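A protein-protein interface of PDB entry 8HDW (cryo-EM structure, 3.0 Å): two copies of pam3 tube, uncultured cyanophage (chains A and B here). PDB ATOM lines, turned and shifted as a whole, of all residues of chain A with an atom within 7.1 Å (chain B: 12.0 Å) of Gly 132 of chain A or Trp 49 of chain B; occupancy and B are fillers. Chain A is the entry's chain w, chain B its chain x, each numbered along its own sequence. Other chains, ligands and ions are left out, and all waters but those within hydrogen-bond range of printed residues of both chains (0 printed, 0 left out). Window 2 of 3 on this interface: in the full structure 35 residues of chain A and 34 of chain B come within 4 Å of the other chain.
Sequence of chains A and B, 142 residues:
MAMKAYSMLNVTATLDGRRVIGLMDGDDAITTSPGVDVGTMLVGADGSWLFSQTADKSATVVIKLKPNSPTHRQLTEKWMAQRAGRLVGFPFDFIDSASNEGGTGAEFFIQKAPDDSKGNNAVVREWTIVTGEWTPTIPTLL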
ATOM      1  N   ALA A  55     -36.363  10.600 -17.980  1.00  0.00           N
ATOM      2  CA  ALA A  55     -34.963  10.243 -18.132  1.00  0.00           C
ATOM      3  C   ALA A  55     -34.024  11.359 -17.693  1.00  0.00           C
ATOM      4  O   ALA A  55     -32.809  11.231 -17.854  1.00  0.00           O
ATOM      5  CB  ALA A  55     -34.680   9.856 -19.581  1.00  0.00           C
ATOM      6  N   ASP A  56     -34.559  12.433 -17.118  1.00  0.00           N
ATOM      7  CA  ASP A  56     -33.779  13.601 -16.714  1.00  0.00           C
ATOM      8  C   ASP A  56     -33.263  13.380 -15.302  1.00  0.00           C
ATOM      9  O   ASP A  56     -34.044  13.275 -14.357  1.00  0.00           O
ATOM     10  CB  ASP A  56     -34.637  14.857 -16.783  1.00  0.00           C
ATOM     11  CG  ASP A  56     -35.796  14.721 -17.757  1.00  0.00           C
ATOM     12  OD1 ASP A  56     -35.941  13.638 -18.365  1.00  0.00           O
ATOM     13  OD2 ASP A  56     -36.571  15.690 -17.916  1.00  0.00           O
ATOM     14  N   LYS A  57     -31.942  13.295 -15.148  1.00  0.00           N
ATOM     15  CA  LYS A  57     -31.328  13.172 -13.827  1.00  0.00           C
ATOM     16  C   LYS A  57     -30.396  14.356 -13.577  1.00  0.00           C
ATOM     17  O   LYS A  57     -29.178  14.249 -13.656  1.00  0.00           O
ATOM     18  CB  LYS A  57     -30.599  11.842 -13.719  1.00  0.00           C
ATOM     19  CG  LYS A  57     -29.825  11.461 -14.949  1.00  0.00           C
ATOM     20  CD  LYS A  57     -29.313  10.046 -14.855  1.00  0.00           C
ATOM     21  CE  LYS A  57     -30.447   9.051 -14.926  1.00  0.00           C
ATOM     22  NZ  LYS A  57     -29.950   7.652 -14.995  1.00  0.00           N
ATOM     23  N   SER A  58     -30.985  15.484 -13.190  1.00  0.00           N
ATOM     24  CA  SER A  58     -30.240  16.717 -12.980  1.00  0.00           C
ATOM     25  C   SER A  58     -30.648  17.336 -11.654  1.00  0.00           C
ATOM     26  O   SER A  58     -31.711  17.036 -11.110  1.00  0.00           O
ATOM     27  CB  SER A  58     -30.471  17.717 -14.111  1.00  0.00           C
ATOM     28  OG  SER A  58     -31.835  18.064 -14.200  1.00  0.00           O
ATOM     29  N   ALA A  59     -29.788  18.211 -11.136  1.00  0.00           N
ATOM     30  CA  ALA A  59     -30.020  18.818  -9.836  1.00  0.00           C
ATOM     31  C   ALA A  59     -29.302  20.154  -9.743  1.00  0.00           C
ATOM     32  O   ALA A  59     -28.381  20.444 -10.506  1.00  0.00           O
ATOM     33  CB  ALA A  59     -29.556  17.899  -8.705  1.00  0.00           C
ATOM     34  N   GLU A 107     -19.532  17.459 -13.317  1.00  0.00           N
ATOM     35  CA  GLU A 107     -19.488  18.700 -14.091  1.00  0.00           C
ATOM     36  C   GLU A 107     -20.591  19.638 -13.622  1.00  0.00           C
ATOM     37  O   GLU A 107     -21.763  19.412 -13.926  1.00  0.00           O
ATOM     38  CB  GLU A 107     -19.631  18.423 -15.586  1.00  0.00           C
ATOM     39  CG  GLU A 107     -18.519  17.584 -16.172  1.00  0.00           C
ATOM     40  CD  GLU A 107     -18.719  17.279 -17.631  1.00  0.00           C
ATOM     41  OE1 GLU A 107     -19.358  18.094 -18.322  1.00  0.00           O
ATOM     42  OE2 GLU A 107     -18.238  16.222 -18.087  1.00  0.00           O
ATOM     43  N   PHE A 108     -20.220  20.700 -12.912  1.00  0.00           N
ATOM     44  CA  PHE A 108     -21.154  21.715 -12.454  1.00  0.00           C
ATOM     45  C   PHE A 108     -20.909  23.038 -13.180  1.00  0.00           C
ATOM     46  O   PHE A 108     -19.932  23.215 -13.898  1.00  0.00           O
ATOM     47  CB  PHE A 108     -21.047  21.885 -10.941  1.00  0.00           C
ATOM     48  CG  PHE A 108     -21.912  20.948 -10.157  1.00  0.00           C
ATOM     49  CD1 PHE A 108     -21.458  19.698  -9.804  1.00  0.00           C
ATOM     50  CD2 PHE A 108     -23.176  21.324  -9.761  1.00  0.00           C
ATOM     51  CE1 PHE A 108     -22.252  18.845  -9.079  1.00  0.00           C
ATOM     52  CE2 PHE A 108     -23.968  20.473  -9.038  1.00  0.00           C
ATOM     53  CZ  PHE A 108     -23.504  19.234  -8.696  1.00  0.00           C
ATOM     54  N   PHE A 109     -21.832  23.978 -13.008  1.00  0.00           N
ATOM     55  CA  PHE A 109     -21.706  25.306 -13.590  1.00  0.00           C
ATOM     56  C   PHE A 109     -22.361  26.307 -12.652  1.00  0.00           C
ATOM     57  O   PHE A 109     -23.314  25.966 -11.954  1.00  0.00           O
ATOM     58  CB  PHE A 109     -22.366  25.395 -14.968  1.00  0.00           C
ATOM     59  CG  PHE A 109     -21.719  24.545 -16.024  1.00  0.00           C
ATOM     60  CD1 PHE A 109     -20.637  25.013 -16.741  1.00  0.00           C
ATOM     61  CD2 PHE A 109     -22.215  23.291 -16.325  1.00  0.00           C
ATOM     62  CE1 PHE A 109     -20.053  24.239 -17.717  1.00  0.00           C
ATOM     63  CE2 PHE A 109     -21.627  22.517 -17.300  1.00  0.00           C
ATOM     64  CZ  PHE A 109     -20.549  22.993 -17.996  1.00  0.00           C
ATOM     65  N   VAL A 130     -25.380  24.154 -10.950  1.00  0.00           N
ATOM     66  CA  VAL A 130     -26.277  23.227 -11.638  1.00  0.00           C
ATOM     67  C   VAL A 130     -25.458  22.181 -12.379  1.00  0.00           C
ATOM     68  O   VAL A 130     -24.388  22.480 -12.914  1.00  0.00           O
ATOM     69  CB  VAL A 130     -27.216  23.971 -12.612  1.00  0.00           C
ATOM     70  CG1 VAL A 130     -28.101  23.011 -13.355  1.00  0.00           C
ATOM     71  CG2 VAL A 130     -28.078  24.924 -11.855  1.00  0.00           C
ATOM     72  N   THR A 131     -25.964  20.952 -12.407  1.00  0.00           N
ATOM     73  CA  THR A 131     -25.366  19.869 -13.171  1.00  0.00           C
ATOM     74  C   THR A 131     -26.429  19.179 -14.014  1.00  0.00           C
ATOM     75  O   THR A 131     -27.627  19.288 -13.754  1.00  0.00           O
ATOM     76  CB  THR A 131     -24.680  18.847 -12.262  1.00  0.00           C
ATOM     77  OG1 THR A 131     -23.951  17.915 -13.063  1.00  0.00           O
ATOM     78  CG2 THR A 131     -25.690  18.096 -11.437  1.00  0.00           C
ATOM     79  N   GLY A 132     -25.972  18.480 -15.046  1.00  0.00           N
ATOM     80  CA  GLY A 132     -26.855  17.696 -15.881  1.00  0.00           C
ATOM     81  C   GLY A 132     -26.950  16.248 -15.455  1.00  0.00           C
ATOM     82  O   GLY A 132     -27.805  15.513 -15.945  1.00  0.00           O
ATOM     83  N   GLU A 133     -26.075  15.824 -14.545  1.00  0.00           N
ATOM     84  CA  GLU A 133     -26.037  14.450 -14.069  1.00  0.00           C
ATOM     85  C   GLU A 133     -25.640  14.418 -12.603  1.00  0.00           C
ATOM     86  O   GLU A 133     -24.512  14.752 -12.244  1.00  0.00           O
ATOM     87  CB  GLU A 133     -25.056  13.609 -14.878  1.00  0.00           C
ATOM     88  CG  GLU A 133     -25.693  12.497 -15.667  1.00  0.00           C
ATOM     89  CD  GLU A 133     -25.468  11.146 -15.039  1.00  0.00           C
ATOM     90  OE1 GLU A 133     -25.833  10.968 -13.862  1.00  0.00           O
ATOM     91  OE2 GLU A 133     -24.917  10.260 -15.722  1.00  0.00           O
ATOM     92  N   TRP A 134     -26.574  13.987 -11.762  1.00  0.00           N
ATOM     93  CA  TRP A 134     -26.354  13.879 -10.325  1.00  0.00           C
ATOM     94  C   TRP A 134     -26.726  12.472  -9.898  1.00  0.00           C
ATOM     95  O   TRP A 134     -27.851  12.031 -10.142  1.00  0.00           O
ATOM     96  CB  TRP A 134     -27.186  14.918  -9.571  1.00  0.00           C
ATOM     97  CG  TRP A 134     -27.236  14.745  -8.089  1.00  0.00           C
ATOM     98  CD1 TRP A 134     -28.195  14.102  -7.377  1.00  0.00           C
ATOM     99  CD2 TRP A 134     -26.299  15.250  -7.133  1.00  0.00           C
ATOM    100  NE1 TRP A 134     -27.911  14.157  -6.040  1.00  0.00           N
ATOM    101  CE2 TRP A 134     -26.751  14.860  -5.864  1.00  0.00           C
ATOM    102  CE3 TRP A 134     -25.119  15.986  -7.229  1.00  0.00           C
ATOM    103  CZ2 TRP A 134     -26.068  15.185  -4.702  1.00  0.00           C
ATOM    104  CZ3 TRP A 134     -24.445  16.306  -6.075  1.00  0.00           C
ATOM    105  CH2 TRP A 134     -24.917  15.906  -4.831  1.00  0.00           C
ATOM    106  N   GLY B  39     -26.615  31.129 -15.965  1.00  0.00           N
ATOM    107  CA  GLY B  39     -26.807  30.148 -17.005  1.00  0.00           C
ATOM    108  C   GLY B  39     -28.070  29.339 -16.813  1.00  0.00           C
ATOM    109  O   GLY B  39     -28.854  29.584 -15.897  1.00  0.00           O
ATOM    110  N   THR B  40     -28.244  28.355 -17.695  1.00  0.00           N
ATOM    111  CA  THR B  40     -29.462  27.556 -17.779  1.00  0.00           C
ATOM    112  C   THR B  40     -29.114  26.143 -18.223  1.00  0.00           C
ATOM    113  O   THR B  40     -28.389  25.965 -19.204  1.00  0.00           O
ATOM    114  CB  THR B  40     -30.454  28.182 -18.766  1.00  0.00           C
ATOM    115  OG1 THR B  40     -30.934  29.426 -18.250  1.00  0.00           O
ATOM    116  CG2 THR B  40     -31.631  27.269 -19.007  1.00  0.00           C
ATOM    117  N   MET B  41     -29.633  25.146 -17.515  1.00  0.00           N
ATOM    118  CA  MET B  41     -29.464  23.748 -17.888  1.00  0.00           C
ATOM    119  C   MET B  41     -30.684  23.274 -18.668  1.00  0.00           C
ATOM    120  O   MET B  41     -31.822  23.523 -18.260  1.00  0.00           O
ATOM    121  CB  MET B  41     -29.254  22.875 -16.650  1.00  0.00           C
ATOM    122  CG  MET B  41     -28.931  21.425 -16.947  1.00  0.00           C
ATOM    123  SD  MET B  41     -27.390  21.201 -17.839  1.00  0.00           S
ATOM    124  CE  MET B  41     -26.216  21.848 -16.663  1.00  0.00           C
ATOM    125  N   LEU B  42     -30.443  22.599 -19.788  1.00  0.00           N
ATOM    126  CA  LEU B  42     -31.491  22.094 -20.667  1.00  0.00           C
ATOM    127  C   LEU B  42     -31.356  20.583 -20.779  1.00  0.00           C
ATOM    128  O   LEU B  42     -30.375  20.088 -21.339  1.00  0.00           O
ATOM    129  CB  LEU B  42     -31.401  22.745 -22.046  1.00  0.00           C
ATOM    130  CG  LEU B  42     -32.157  22.100 -23.211  1.00  0.00           C
ATOM    131  CD1 LEU B  42     -33.652  22.312 -23.086  1.00  0.00           C
ATOM    132  CD2 LEU B  42     -31.642  22.633 -24.538  1.00  0.00           C
ATOM    133  N   VAL B  43     -32.341  19.857 -20.261  1.00  0.00           N
ATOM    134  CA  VAL B  43     -32.325  18.399 -20.232  1.00  0.00           C
ATOM    135  C   VAL B  43     -33.379  17.882 -21.199  1.00  0.00           C
ATOM    136  O   VAL B  43     -34.526  18.339 -21.178  1.00  0.00           O
ATOM    137  CB  VAL B  43     -32.568  17.864 -18.812  1.00  0.00           C
ATOM    138  CG1 VAL B  43     -32.359  16.373 -18.774  1.00  0.00           C
ATOM    139  CG2 VAL B  43     -31.644  18.549 -17.835  1.00  0.00           C
ATOM    140  N   GLY B  44     -32.989  16.932 -22.046  1.00  0.00           N
ATOM    141  CA  GLY B  44     -33.867  16.419 -23.073  1.00  0.00           C
ATOM    142  C   GLY B  44     -34.667  15.208 -22.637  1.00  0.00           C
ATOM    143  O   GLY B  44     -34.559  14.709 -21.517  1.00  0.00           O
ATOM    144  N   ALA B  45     -35.491  14.720 -23.566  1.00  0.00           N
ATOM    145  CA  ALA B  45     -36.378  13.597 -23.289  1.00  0.00           C
ATOM    146  C   ALA B  45     -35.633  12.290 -23.091  1.00  0.00           C
ATOM    147  O   ALA B  45     -36.237  11.316 -22.636  1.00  0.00           O
ATOM    148  CB  ALA B  45     -37.395  13.441 -24.416  1.00  0.00           C
ATOM    149  N   ASP B  46     -34.344  12.247 -23.412  1.00  0.00           N
ATOM    150  CA  ASP B  46     -33.558  11.028 -23.324  1.00  0.00           C
ATOM    151  C   ASP B  46     -32.614  10.999 -22.131  1.00  0.00           C
ATOM    152  O   ASP B  46     -32.040   9.945 -21.843  1.00  0.00           O
ATOM    153  CB  ASP B  46     -32.742  10.842 -24.607  1.00  0.00           C
ATOM    154  CG  ASP B  46     -32.439   9.394 -24.891  1.00  0.00           C
ATOM    155  OD1 ASP B  46     -32.905   8.535 -24.114  1.00  0.00           O
ATOM    156  OD2 ASP B  46     -31.742   9.111 -25.889  1.00  0.00           O
ATOM    157  N   GLY B  47     -32.433  12.119 -21.441  1.00  0.00           N
ATOM    158  CA  GLY B  47     -31.519  12.204 -20.319  1.00  0.00           C
ATOM    159  C   GLY B  47     -30.254  12.984 -20.589  1.00  0.00           C
ATOM    160  O   GLY B  47     -29.520  13.283 -19.637  1.00  0.00           O
ATOM    161  N   SER B  48     -29.958  13.321 -21.839  1.00  0.00           N
ATOM    162  CA  SER B  48     -28.812  14.150 -22.158  1.00  0.00           C
ATOM    163  C   SER B  48     -29.097  15.604 -21.790  1.00  0.00           C
ATOM    164  O   SER B  48     -30.243  16.005 -21.584  1.00  0.00           O
ATOM    165  CB  SER B  48     -28.466  14.019 -23.636  1.00  0.00           C
ATOM    166  OG  SER B  48     -29.628  14.144 -24.428  1.00  0.00           O
ATOM    167  N   TRP B  49     -28.038  16.405 -21.708  1.00  0.00           N
ATOM    168  CA  TRP B  49     -28.154  17.753 -21.173  1.00  0.00           C
ATOM    169  C   TRP B  49     -27.259  18.718 -21.936  1.00  0.00           C
ATOM    170  O   TRP B  49     -26.338  18.310 -22.644  1.00  0.00           O
ATOM    171  CB  TRP B  49     -27.812  17.779 -19.683  1.00  0.00           C
ATOM    172  CG  TRP B  49     -26.530  17.103 -19.337  1.00  0.00           C
ATOM    173  CD1 TRP B  49     -26.349  15.787 -19.075  1.00  0.00           C
ATOM    174  CD2 TRP B  49     -25.247  17.719 -19.199  1.00  0.00           C
ATOM    175  NE1 TRP B  49     -25.035  15.534 -18.789  1.00  0.00           N
ATOM    176  CE2 TRP B  49     -24.336  16.707 -18.859  1.00  0.00           C
ATOM    177  CE3 TRP B  49     -24.782  19.031 -19.332  1.00  0.00           C
ATOM    178  CZ2 TRP B  49     -22.988  16.961 -18.652  1.00  0.00           C
ATOM    179  CZ3 TRP B  49     -23.447  19.281 -19.129  1.00  0.00           C
ATOM    180  CH2 TRP B  49     -22.564  18.252 -18.791  1.00  0.00           C
ATOM    181  N   LEU B  50     -27.556  20.007 -21.790  1.00  0.00           N
ATOM    182  CA  LEU B  50     -26.761  21.069 -22.389  1.00  0.00           C
ATOM    183  C   LEU B  50     -26.875  22.316 -21.525  1.00  0.00           C
ATOM    184  O   LEU B  50     -27.982  22.719 -21.167  1.00  0.00           O
ATOM    185  CB  LEU B  50     -27.225  21.365 -23.816  1.00  0.00           C
ATOM    186  CG  LEU B  50     -26.516  22.480 -24.583  1.00  0.00           C
ATOM    187  CD1 LEU B  50     -25.050  22.175 -24.756  1.00  0.00           C
ATOM    188  CD2 LEU B  50     -27.168  22.676 -25.923  1.00  0.00           C
ATOM    189  N   PHE B  51     -25.739  22.917 -21.196  1.00  0.00           N
ATOM    190  CA  PHE B  51     -25.679  24.157 -20.436  1.00  0.00           C
ATOM    191  C   PHE B  51     -25.480  25.326 -21.391  1.00  0.00           C
ATOM    192  O   PHE B  51     -24.867  25.175 -22.447  1.00  0.00           O
ATOM    193  CB  PHE B  51     -24.540  24.094 -19.415  1.00  0.00           C
ATOM    194  CG  PHE B  51     -24.434  25.304 -18.533  1.00  0.00           C
ATOM    195  CD1 PHE B  51     -25.330  25.509 -17.504  1.00  0.00           C
ATOM    196  CD2 PHE B  51     -23.415  26.222 -18.714  1.00  0.00           C
ATOM    197  CE1 PHE B  51     -25.225  26.613 -16.689  1.00  0.00           C
ATOM    198  CE2 PHE B  51     -23.310  27.329 -17.898  1.00  0.00           C
ATOM    199  CZ  PHE B  51     -24.213  27.522 -16.888  1.00  0.00           C
ATOM    200  N   SER B  52     -26.020  26.487 -21.038  1.00  0.00           N
ATOM    201  CA  SER B  52     -25.824  27.693 -21.831  1.00  0.00           C
ATOM    202  C   SER B  52     -25.542  28.868 -20.908  1.00  0.00           C
ATOM    203  O   SER B  52     -26.246  29.066 -19.916  1.00  0.00           O
ATOM    204  CB  SER B  52     -27.032  27.982 -22.724  1.00  0.00           C
ATOM    205  OG  SER B  52     -28.161  28.337 -21.962  1.00  0.00           O
ATOM    206  N   GLN B  53     -24.517  29.645 -21.245  1.00  0.00           N
ATOM    207  CA  GLN B  53     -24.037  30.747 -20.426  1.00  0.00           C
ATOM    208  C   GLN B  53     -24.351  32.068 -21.113  1.00  0.00           C
ATOM    209  O   GLN B  53     -24.227  32.180 -22.335  1.00  0.00           O
ATOM    210  CB  GLN B  53     -22.533  30.615 -20.188  1.00  0.00           C
ATOM    211  CG  GLN B  53     -22.081  30.978 -18.790  1.00  0.00           C
ATOM    212  CD  GLN B  53     -21.539  32.368 -18.711  1.00  0.00           C
ATOM    213  OE1 GLN B  53     -21.045  32.901 -19.694  1.00  0.00           O
ATOM    214  NE2 GLN B  53     -21.629  32.973 -17.541  1.00  0.00           N
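The side-chain hydroxyl of Thr 131 of chain A lies within hydrogen-bond range of the backbone carbonyl oxygen of Glu 133 of chain A (3.3 Å). O of Glu 107 of chain A sits at hydrogen-bond distance from OG1 of Thr 131 of chain A (2.8 Å). The backbone carbonyl oxygen (O) of Phe 109 of chain A sits at hydrogen-bond distance from the backbone NH (N) of Val 130 of chain A, at 2.9 Å. The backbone carbonyl oxygen (O) of Ala 59 of chain A sits at hydrogen-bond distance from the backbone NH (N) of Thr 131 of chain A (3.1 Å).
Printed residues of chain B that touch a printed residue of chain A: Met 41, Val 43, Gly 44, Ala 45, Asp 46, Gly 47, Trp 49 and Phe 51. Hydrophobic or aromatic side chains of chain B within 4 Å of the printed part of chain A: Met 41, Val 43, Trp 49 and Phe 51. Of the 13 printed residues of chain A, 8 touch a printed residue of chain B. Printed residues of chain A that touch a printed residue of chain B: Ala 55, Asp 56, Ser 58, Glu 107, Phe 109, Val 130, Thr 131 and Gly 132.
No position is printed for both chains. Of the 12 pairs that touch across the chains among the printed residues, none has its exchanged pair printed and touching as well.
Among the printed residues, pairs that only touch across the chains: Ala 55 of chain A with Ala 45 of chain B (3.7 Å), Ala 55 of chain A with Asp 46 of chain B (3.5 Å), Ala 55 of chain A with Gly 47 of chain B (2.9 Å), Asp 56 of chain A with Val 43 of chain B (3.4 Å), Asp 56 of chain A with Gly 44 of chain B (3.6 Å), Ser 58 of chain A with Val 43 of chain B (3.7 Å), Glu 107 of chain A with Trp 49 of chain B (3.2 Å), Phe 109 of chain A with Phe 51 of chain B (3.4 Å), Val 130 of chain A with Met 41 of chain B (3.5 Å), Thr 131 of chain A with Met 41 of chain B (3.8 Å), Gly 132 of chain A with Met 41 of chain B (3.7 Å) and Gly 132 of chain A with Trp 49 of chain B (3.5 Å).
Of the printed residues of chain B, Ala 55 of chain A touches Ala 45, Asp 46 and Gly 47. Ser 58 of chain A touches just one residue of chain B: Val 43 (3.7 Å). No residue of chain B comes within 4 Å of Ala 59 of chain A. Glu 107 of chain A touches one residue of chain B. No residue of chain B comes within 4 Å of Phe 108 of chain A. Gly 132 of chain A touches just these residues of chain B: Met 41 (3.7 Å) and Trp 49 (3.5 Å). No residue of chain B comes within 4 Å of Glu 133 of chain A. Of the printed residues of chain A, Met 41 of chain B touches Val 130 (3.5 Å), Thr 131 (3.8 Å) and Gly 132 (3.7 Å). Of the printed residues of chain A, Gly 44 of chain B touches Asp 56. Printed residues of chain A within 4 Å of Ala 45 of chain B: Ala 55. Printed residues of chain A within 4 Å of Asp 46 of chain B: Ala 55 (3.5 Å). Printed residues of chain A within 4 Å of Trp 49 of chain B: Glu 107 (3.2 Å) and Gly 132 (3.5 Å). The nearest residue of chain B that does not touch Gly 132 of chain A is Gly 47 of chain B (4.6 Å). The nearest residue of chain A that does not touch Trp 49 of chain B is Phe 109 of chain A (4.1 Å).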
